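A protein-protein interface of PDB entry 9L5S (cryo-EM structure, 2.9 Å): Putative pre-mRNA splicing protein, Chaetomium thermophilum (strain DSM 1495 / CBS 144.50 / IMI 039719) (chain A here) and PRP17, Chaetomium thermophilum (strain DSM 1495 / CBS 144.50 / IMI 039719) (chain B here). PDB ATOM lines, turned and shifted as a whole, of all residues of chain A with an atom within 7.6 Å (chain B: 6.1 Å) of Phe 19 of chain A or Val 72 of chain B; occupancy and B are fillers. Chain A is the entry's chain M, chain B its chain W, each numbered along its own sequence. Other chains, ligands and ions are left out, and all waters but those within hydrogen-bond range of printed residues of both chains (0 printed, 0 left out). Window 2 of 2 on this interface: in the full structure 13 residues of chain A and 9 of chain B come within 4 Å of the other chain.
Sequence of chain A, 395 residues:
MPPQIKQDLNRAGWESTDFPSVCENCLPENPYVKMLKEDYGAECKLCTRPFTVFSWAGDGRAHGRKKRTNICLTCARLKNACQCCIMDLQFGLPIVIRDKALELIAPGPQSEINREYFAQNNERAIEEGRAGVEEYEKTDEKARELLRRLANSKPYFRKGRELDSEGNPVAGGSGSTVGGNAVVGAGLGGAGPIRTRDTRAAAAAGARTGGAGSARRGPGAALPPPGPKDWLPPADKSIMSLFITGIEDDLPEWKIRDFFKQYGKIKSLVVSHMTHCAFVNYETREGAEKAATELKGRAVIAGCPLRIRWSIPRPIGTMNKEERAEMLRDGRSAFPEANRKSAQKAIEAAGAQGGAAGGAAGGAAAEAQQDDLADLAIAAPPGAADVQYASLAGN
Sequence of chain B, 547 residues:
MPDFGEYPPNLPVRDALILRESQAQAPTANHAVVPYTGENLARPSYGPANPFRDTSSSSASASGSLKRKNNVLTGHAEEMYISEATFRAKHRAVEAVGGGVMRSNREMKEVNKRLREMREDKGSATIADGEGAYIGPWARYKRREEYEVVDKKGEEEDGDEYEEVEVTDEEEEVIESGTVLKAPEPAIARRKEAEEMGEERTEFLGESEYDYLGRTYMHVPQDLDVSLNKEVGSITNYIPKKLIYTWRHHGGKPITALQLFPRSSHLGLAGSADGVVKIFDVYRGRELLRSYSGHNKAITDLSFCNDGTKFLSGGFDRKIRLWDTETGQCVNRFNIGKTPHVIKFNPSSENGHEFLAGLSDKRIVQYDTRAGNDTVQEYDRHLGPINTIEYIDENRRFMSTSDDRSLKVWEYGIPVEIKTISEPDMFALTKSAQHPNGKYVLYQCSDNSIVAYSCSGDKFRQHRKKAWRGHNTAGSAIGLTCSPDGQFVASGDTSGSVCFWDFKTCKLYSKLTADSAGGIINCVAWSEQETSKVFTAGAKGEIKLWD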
ATOM      1  N   ASP A  18     -33.992 -29.105  10.244  1.00  0.00           N
ATOM      2  CA  ASP A  18     -34.535 -27.920  10.898  1.00  0.00           C
ATOM      3  C   ASP A  18     -33.419 -26.962  11.298  1.00  0.00           C
ATOM      4  O   ASP A  18     -33.657 -25.966  11.979  1.00  0.00           O
ATOM      5  CB  ASP A  18     -35.358 -28.313  12.126  1.00  0.00           C
ATOM      6  CG  ASP A  18     -36.716 -28.878  11.759  1.00  0.00           C
ATOM      7  OD1 ASP A  18     -37.274 -28.460  10.724  1.00  0.00           O
ATOM      8  OD2 ASP A  18     -37.224 -29.743  12.503  1.00  0.00           O
ATOM      9  N   PHE A  19     -32.196 -27.272  10.866  1.00  0.00           N
ATOM     10  CA  PHE A  19     -31.036 -26.452  11.162  1.00  0.00           C
ATOM     11  C   PHE A  19     -30.097 -26.505   9.968  1.00  0.00           C
ATOM     12  O   PHE A  19     -29.856 -27.595   9.429  1.00  0.00           O
ATOM     13  CB  PHE A  19     -30.315 -26.929  12.427  1.00  0.00           C
ATOM     14  CG  PHE A  19     -29.267 -25.980  12.918  1.00  0.00           C
ATOM     15  CD1 PHE A  19     -29.621 -24.788  13.529  1.00  0.00           C
ATOM     16  CD2 PHE A  19     -27.925 -26.273  12.760  1.00  0.00           C
ATOM     17  CE1 PHE A  19     -28.654 -23.911  13.974  1.00  0.00           C
ATOM     18  CE2 PHE A  19     -26.957 -25.400  13.200  1.00  0.00           C
ATOM     19  CZ  PHE A  19     -27.320 -24.220  13.810  1.00  0.00           C
ATOM     20  N   PRO A  20     -29.559 -25.370   9.535  1.00  0.00           N
ATOM     21  CA  PRO A  20     -28.691 -25.362   8.356  1.00  0.00           C
ATOM     22  C   PRO A  20     -27.298 -25.892   8.663  1.00  0.00           C
ATOM     23  O   PRO A  20     -26.879 -26.002   9.816  1.00  0.00           O
ATOM     24  CB  PRO A  20     -28.640 -23.878   7.984  1.00  0.00           C
ATOM     25  CG  PRO A  20     -28.739 -23.201   9.307  1.00  0.00           C
ATOM     26  CD  PRO A  20     -29.772 -24.008  10.050  1.00  0.00           C
ATOM     27  N   SER A  21     -26.577 -26.213   7.595  1.00  0.00           N
ATOM     28  CA  SER A  21     -25.194 -26.672   7.683  1.00  0.00           C
ATOM     29  C   SER A  21     -24.336 -25.572   7.068  1.00  0.00           C
ATOM     30  O   SER A  21     -24.049 -25.578   5.870  1.00  0.00           O
ATOM     31  CB  SER A  21     -25.000 -28.002   6.972  1.00  0.00           C
ATOM     32  OG  SER A  21     -25.247 -27.876   5.586  1.00  0.00           O
ATOM     33  N   VAL A  22     -23.931 -24.622   7.902  1.00  0.00           N
ATOM     34  CA  VAL A  22     -23.252 -23.412   7.461  1.00  0.00           C
ATOM     35  C   VAL A  22     -21.906 -23.337   8.164  1.00  0.00           C
ATOM     36  O   VAL A  22     -21.823 -23.549   9.378  1.00  0.00           O
ATOM     37  CB  VAL A  22     -24.104 -22.159   7.737  1.00  0.00           C
ATOM     38  CG1 VAL A  22     -23.361 -20.899   7.319  1.00  0.00           C
ATOM     39  CG2 VAL A  22     -25.434 -22.254   7.005  1.00  0.00           C
ATOM     40  N   LEU A  27     -20.852 -17.740   8.882  1.00  0.00           N
ATOM     41  CA  LEU A  27     -21.614 -17.321  10.037  1.00  0.00           C
ATOM     42  C   LEU A  27     -21.063 -15.997  10.566  1.00  0.00           C
ATOM     43  O   LEU A  27     -19.911 -15.646  10.297  1.00  0.00           O
ATOM     44  CB  LEU A  27     -21.561 -18.404  11.113  1.00  0.00           C
ATOM     45  CG  LEU A  27     -22.623 -19.502  10.998  1.00  0.00           C
ATOM     46  CD1 LEU A  27     -22.489 -20.494  12.138  1.00  0.00           C
ATOM     47  CD2 LEU A  27     -24.026 -18.926  10.951  1.00  0.00           C
ATOM     48  N   MET A  35     -31.354 -15.471  13.423  1.00  0.00           N
ATOM     49  CA  MET A  35     -31.533 -16.170  12.160  1.00  0.00           C
ATOM     50  C   MET A  35     -33.011 -16.236  11.796  1.00  0.00           C
ATOM     51  O   MET A  35     -33.855 -16.546  12.640  1.00  0.00           O
ATOM     52  CB  MET A  35     -30.940 -17.582  12.246  1.00  0.00           C
ATOM     53  CG  MET A  35     -30.949 -18.366  10.951  1.00  0.00           C
ATOM     54  SD  MET A  35     -30.018 -19.901  11.115  1.00  0.00           S
ATOM     55  CE  MET A  35     -28.342 -19.308  10.919  1.00  0.00           C
ATOM     56  N   LYS A  37     -35.947 -18.000   9.296  1.00  0.00           N
ATOM     57  CA  LYS A  37     -36.198 -19.297   8.680  1.00  0.00           C
ATOM     58  C   LYS A  37     -37.483 -19.228   7.872  1.00  0.00           C
ATOM     59  O   LYS A  37     -38.528 -18.829   8.395  1.00  0.00           O
ATOM     60  CB  LYS A  37     -36.292 -20.396   9.743  1.00  0.00           C
ATOM     61  CG  LYS A  37     -37.011 -21.651   9.288  1.00  0.00           C
ATOM     62  CD  LYS A  37     -37.303 -22.571  10.457  1.00  0.00           C
ATOM     63  CE  LYS A  37     -38.118 -23.775  10.019  1.00  0.00           C
ATOM     64  NZ  LYS A  37     -38.291 -24.760  11.120  1.00  0.00           N
ATOM     65  N   THR A  52     -36.166 -25.248   2.816  1.00  0.00           N
ATOM     66  CA  THR A  52     -36.209 -24.283   3.908  1.00  0.00           C
ATOM     67  C   THR A  52     -34.951 -23.424   3.895  1.00  0.00           C
ATOM     68  O   THR A  52     -33.837 -23.938   4.026  1.00  0.00           O
ATOM     69  CB  THR A  52     -36.348 -25.006   5.245  1.00  0.00           C
ATOM     70  OG1 THR A  52     -37.557 -25.775   5.251  1.00  0.00           O
ATOM     71  CG2 THR A  52     -36.382 -24.008   6.386  1.00  0.00           C
ATOM     72  N   PHE A  54     -32.540 -20.581   5.450  1.00  0.00           N
ATOM     73  CA  PHE A  54     -32.118 -19.890   6.658  1.00  0.00           C
ATOM     74  C   PHE A  54     -31.271 -18.694   6.257  1.00  0.00           C
ATOM     75  O   PHE A  54     -30.407 -18.803   5.384  1.00  0.00           O
ATOM     76  CB  PHE A  54     -31.323 -20.820   7.578  1.00  0.00           C
ATOM     77  CG  PHE A  54     -32.161 -21.868   8.248  1.00  0.00           C
ATOM     78  CD1 PHE A  54     -32.459 -23.053   7.596  1.00  0.00           C
ATOM     79  CD2 PHE A  54     -32.663 -21.666   9.521  1.00  0.00           C
ATOM     80  CE1 PHE A  54     -33.230 -24.020   8.206  1.00  0.00           C
ATOM     81  CE2 PHE A  54     -33.438 -22.631  10.135  1.00  0.00           C
ATOM     82  CZ  PHE A  54     -33.722 -23.808   9.475  1.00  0.00           C
ATOM     83  N   THR A  69     -28.724 -19.625   3.077  1.00  0.00           N
ATOM     84  CA  THR A  69     -28.442 -20.946   2.535  1.00  0.00           C
ATOM     85  C   THR A  69     -28.876 -20.981   1.076  1.00  0.00           C
ATOM     86  O   THR A  69     -30.070 -20.880   0.777  1.00  0.00           O
ATOM     87  CB  THR A  69     -29.171 -22.020   3.337  1.00  0.00           C
ATOM     88  OG1 THR A  69     -30.583 -21.872   3.159  1.00  0.00           O
ATOM     89  CG2 THR A  69     -28.840 -21.899   4.812  1.00  0.00           C
ATOM     90  N   LEU A  73     -30.164 -29.047   1.841  1.00  0.00           N
ATOM     91  CA  LEU A  73     -29.314 -29.854   2.708  1.00  0.00           C
ATOM     92  C   LEU A  73     -28.898 -31.159   2.037  1.00  0.00           C
ATOM     93  O   LEU A  73     -27.792 -31.654   2.278  1.00  0.00           O
ATOM     94  CB  LEU A  73     -30.033 -30.127   4.029  1.00  0.00           C
ATOM     95  CG  LEU A  73     -29.195 -30.701   5.171  1.00  0.00           C
ATOM     96  CD1 LEU A  73     -28.003 -29.811   5.463  1.00  0.00           C
ATOM     97  CD2 LEU A  73     -30.047 -30.879   6.413  1.00  0.00           C
ATOM     98  N   ARG A  77     -25.146 -32.419   1.389  1.00  0.00           N
ATOM     99  CA  ARG A  77     -24.539 -33.699   1.731  1.00  0.00           C
ATOM    100  C   ARG A  77     -23.862 -34.328   0.522  1.00  0.00           C
ATOM    101  O   ARG A  77     -22.793 -34.935   0.651  1.00  0.00           O
ATOM    102  CB  ARG A  77     -25.577 -34.670   2.290  1.00  0.00           C
ATOM    103  CG  ARG A  77     -26.159 -34.304   3.633  1.00  0.00           C
ATOM    104  CD  ARG A  77     -27.156 -35.362   4.046  1.00  0.00           C
ATOM    105  NE  ARG A  77     -27.759 -35.104   5.346  1.00  0.00           N
ATOM    106  CZ  ARG A  77     -28.879 -34.419   5.522  1.00  0.00           C
ATOM    107  NH1 ARG A  77     -29.580 -33.969   4.495  1.00  0.00           N
ATOM    108  NH2 ARG A  77     -29.319 -34.200   6.757  1.00  0.00           N
ATOM    109  N   GLN A  83     -23.874 -24.512   2.867  1.00  0.00           N
ATOM    110  CA  GLN A  83     -25.087 -24.135   2.156  1.00  0.00           C
ATOM    111  C   GLN A  83     -25.046 -22.697   1.656  1.00  0.00           C
ATOM    112  O   GLN A  83     -25.807 -22.350   0.747  1.00  0.00           O
ATOM    113  CB  GLN A  83     -26.295 -24.348   3.065  1.00  0.00           C
ATOM    114  CG  GLN A  83     -26.889 -25.740   2.983  1.00  0.00           C
ATOM    115  CD  GLN A  83     -28.160 -25.871   3.791  1.00  0.00           C
ATOM    116  OE1 GLN A  83     -28.116 -26.080   5.003  1.00  0.00           O
ATOM    117  NE2 GLN A  83     -29.300 -25.746   3.127  1.00  0.00           N
ATOM    118  N   ASN B  70     -21.589 -35.549  15.615  1.00  0.00           N
ATOM    119  CA  ASN B  70     -22.188 -34.287  15.189  1.00  0.00           C
ATOM    120  C   ASN B  70     -23.584 -34.491  14.606  1.00  0.00           C
ATOM    121  O   ASN B  70     -23.806 -35.384  13.784  1.00  0.00           O
ATOM    122  CB  ASN B  70     -21.283 -33.618  14.157  1.00  0.00           C
ATOM    123  CG  ASN B  70     -19.963 -33.166  14.745  1.00  0.00           C
ATOM    124  OD1 ASN B  70     -19.684 -33.399  15.921  1.00  0.00           O
ATOM    125  ND2 ASN B  70     -19.140 -32.520  13.929  1.00  0.00           N
ATOM    126  N   ASN B  71     -24.527 -33.650  15.045  1.00  0.00           N
ATOM    127  CA  ASN B  71     -25.917 -33.797  14.626  1.00  0.00           C
ATOM    128  C   ASN B  71     -26.102 -33.342  13.180  1.00  0.00           C
ATOM    129  O   ASN B  71     -26.771 -34.020  12.392  1.00  0.00           O
ATOM    130  CB  ASN B  71     -26.822 -33.005  15.577  1.00  0.00           C
ATOM    131  CG  ASN B  71     -28.312 -33.269  15.360  1.00  0.00           C
ATOM    132  OD1 ASN B  71     -28.715 -34.030  14.480  1.00  0.00           O
ATOM    133  ND2 ASN B  71     -29.137 -32.628  16.178  1.00  0.00           N
ATOM    134  N   VAL B  72     -25.505 -32.215  12.808  1.00  0.00           N
ATOM    135  CA  VAL B  72     -25.596 -31.699  11.452  1.00  0.00           C
ATOM    136  C   VAL B  72     -24.240 -31.868  10.774  1.00  0.00           C
ATOM    137  O   VAL B  72     -23.276 -32.351  11.368  1.00  0.00           O
ATOM    138  CB  VAL B  72     -26.069 -30.230  11.409  1.00  0.00           C
ATOM    139  CG1 VAL B  72     -27.393 -30.073  12.137  1.00  0.00           C
ATOM    140  CG2 VAL B  72     -25.019 -29.295  11.980  1.00  0.00           C
ATOM    141  N   LEU B  73     -24.181 -31.476   9.499  1.00  0.00           N
ATOM    142  CA  LEU B  73     -23.003 -31.727   8.677  1.00  0.00           C
ATOM    143  C   LEU B  73     -21.797 -30.898   9.103  1.00  0.00           C
ATOM    144  O   LEU B  73     -20.660 -31.291   8.822  1.00  0.00           O
ATOM    145  CB  LEU B  73     -23.349 -31.454   7.211  1.00  0.00           C
ATOM    146  CG  LEU B  73     -22.495 -32.018   6.072  1.00  0.00           C
ATOM    147  CD1 LEU B  73     -23.393 -32.244   4.892  1.00  0.00           C
ATOM    148  CD2 LEU B  73     -21.371 -31.090   5.662  1.00  0.00           C
ATOM    149  N   THR B  74     -22.008 -29.783   9.802  1.00  0.00           N
ATOM    150  CA  THR B  74     -20.924 -28.871  10.125  1.00  0.00           C
ATOM    151  C   THR B  74     -20.577 -28.883  11.610  1.00  0.00           C
ATOM    152  O   THR B  74     -19.445 -28.543  11.973  1.00  0.00           O
ATOM    153  CB  THR B  74     -21.305 -27.447   9.674  1.00  0.00           C
ATOM    154  OG1 THR B  74     -21.755 -27.496   8.316  1.00  0.00           O
ATOM    155  CG2 THR B  74     -20.106 -26.509   9.692  1.00  0.00           C
ATOM    156  N   GLY B  75     -21.483 -29.341  12.458  1.00  0.00           N
ATOM    157  CA  GLY B  75     -21.211 -29.407  13.874  1.00  0.00           C
ATOM    158  C   GLY B  75     -22.313 -30.139  14.600  1.00  0.00           C
ATOM    159  O   GLY B  75     -23.065 -30.909  14.003  1.00  0.00           O
ATOM    160  N   HIS B  76     -22.398 -29.898  15.904  1.00  0.00           N
ATOM    161  CA  HIS B  76     -23.448 -30.469  16.733  1.00  0.00           C
ATOM    162  C   HIS B  76     -24.376 -29.358  17.199  1.00  0.00           C
ATOM    163  O   HIS B  76     -23.926 -28.387  17.816  1.00  0.00           O
ATOM    164  CB  HIS B  76     -22.864 -31.214  17.935  1.00  0.00           C
ATOM    165  CG  HIS B  76     -23.901 -31.798  18.841  1.00  0.00           C
ATOM    166  ND1 HIS B  76     -24.832 -32.717  18.409  1.00  0.00           N
ATOM    167  CD2 HIS B  76     -24.154 -31.596  20.156  1.00  0.00           C
ATOM    168  CE1 HIS B  76     -25.615 -33.055  19.417  1.00  0.00           C
ATOM    169  NE2 HIS B  76     -25.224 -32.389  20.489  1.00  0.00           N
ATOM    170  N   ALA B  77     -25.665 -29.504  16.904  1.00  0.00           N
ATOM    171  CA  ALA B  77     -26.669 -28.509  17.250  1.00  0.00           C
ATOM    172  C   ALA B  77     -27.804 -29.183  18.003  1.00  0.00           C
ATOM    173  O   ALA B  77     -28.365 -30.175  17.527  1.00  0.00           O
ATOM    174  CB  ALA B  77     -27.205 -27.809  15.998  1.00  0.00           C
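The side-chain amide nitrogen (ND2) of Asn 71 of chain B sits at hydrogen-bond distance from the backbone carbonyl oxygen (O) of Ala 77 of chain B.
The backbone NH (N) of Ser 21 of chain A sits at hydrogen-bond distance from the side-chain amide oxygen (OE1) of Gln 83 of chain A, 3.0 Å away.
Phe 19 of chain A touches just these residues of chain B: Val 72 and Ala 77.
Printed residues of chain B within 4 Å of Val 22 of chain A: Thr 74 (3.4 Å).
Val 72 of chain B touches one residue of chain A.
Printed residues of chain A within 4 Å of Thr 74 of chain B: Ser 21 and Val 22.
Gly 75 of chain B touches none of the printed residues of chain A.
Hydrophobic or aromatic side chains of chain A that line the printed part of chain B: Phe 19.
Hydrophobic or aromatic side chains of chain B that line the printed part of chain A: Val 72, Leu 73 and Ala 77.
Among the printed residues, 6 pairs touch across the chains.
Among the printed residues, pairs that only touch across the chains: Val 22 of chain A with Thr 74 of chain B (3.4 Å), Ser 21 of chain A with Thr 74 of chain B (3.5 Å), Phe 19 of chain A with Ala 77 of chain B (3.7 Å), Arg 77 of chain A with Leu 73 of chain B (3.7 Å), Ser 21 of chain A with Leu 73 of chain B (3.8 Å) and Phe 19 of chain A with Val 72 of chain B (3.9 Å).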
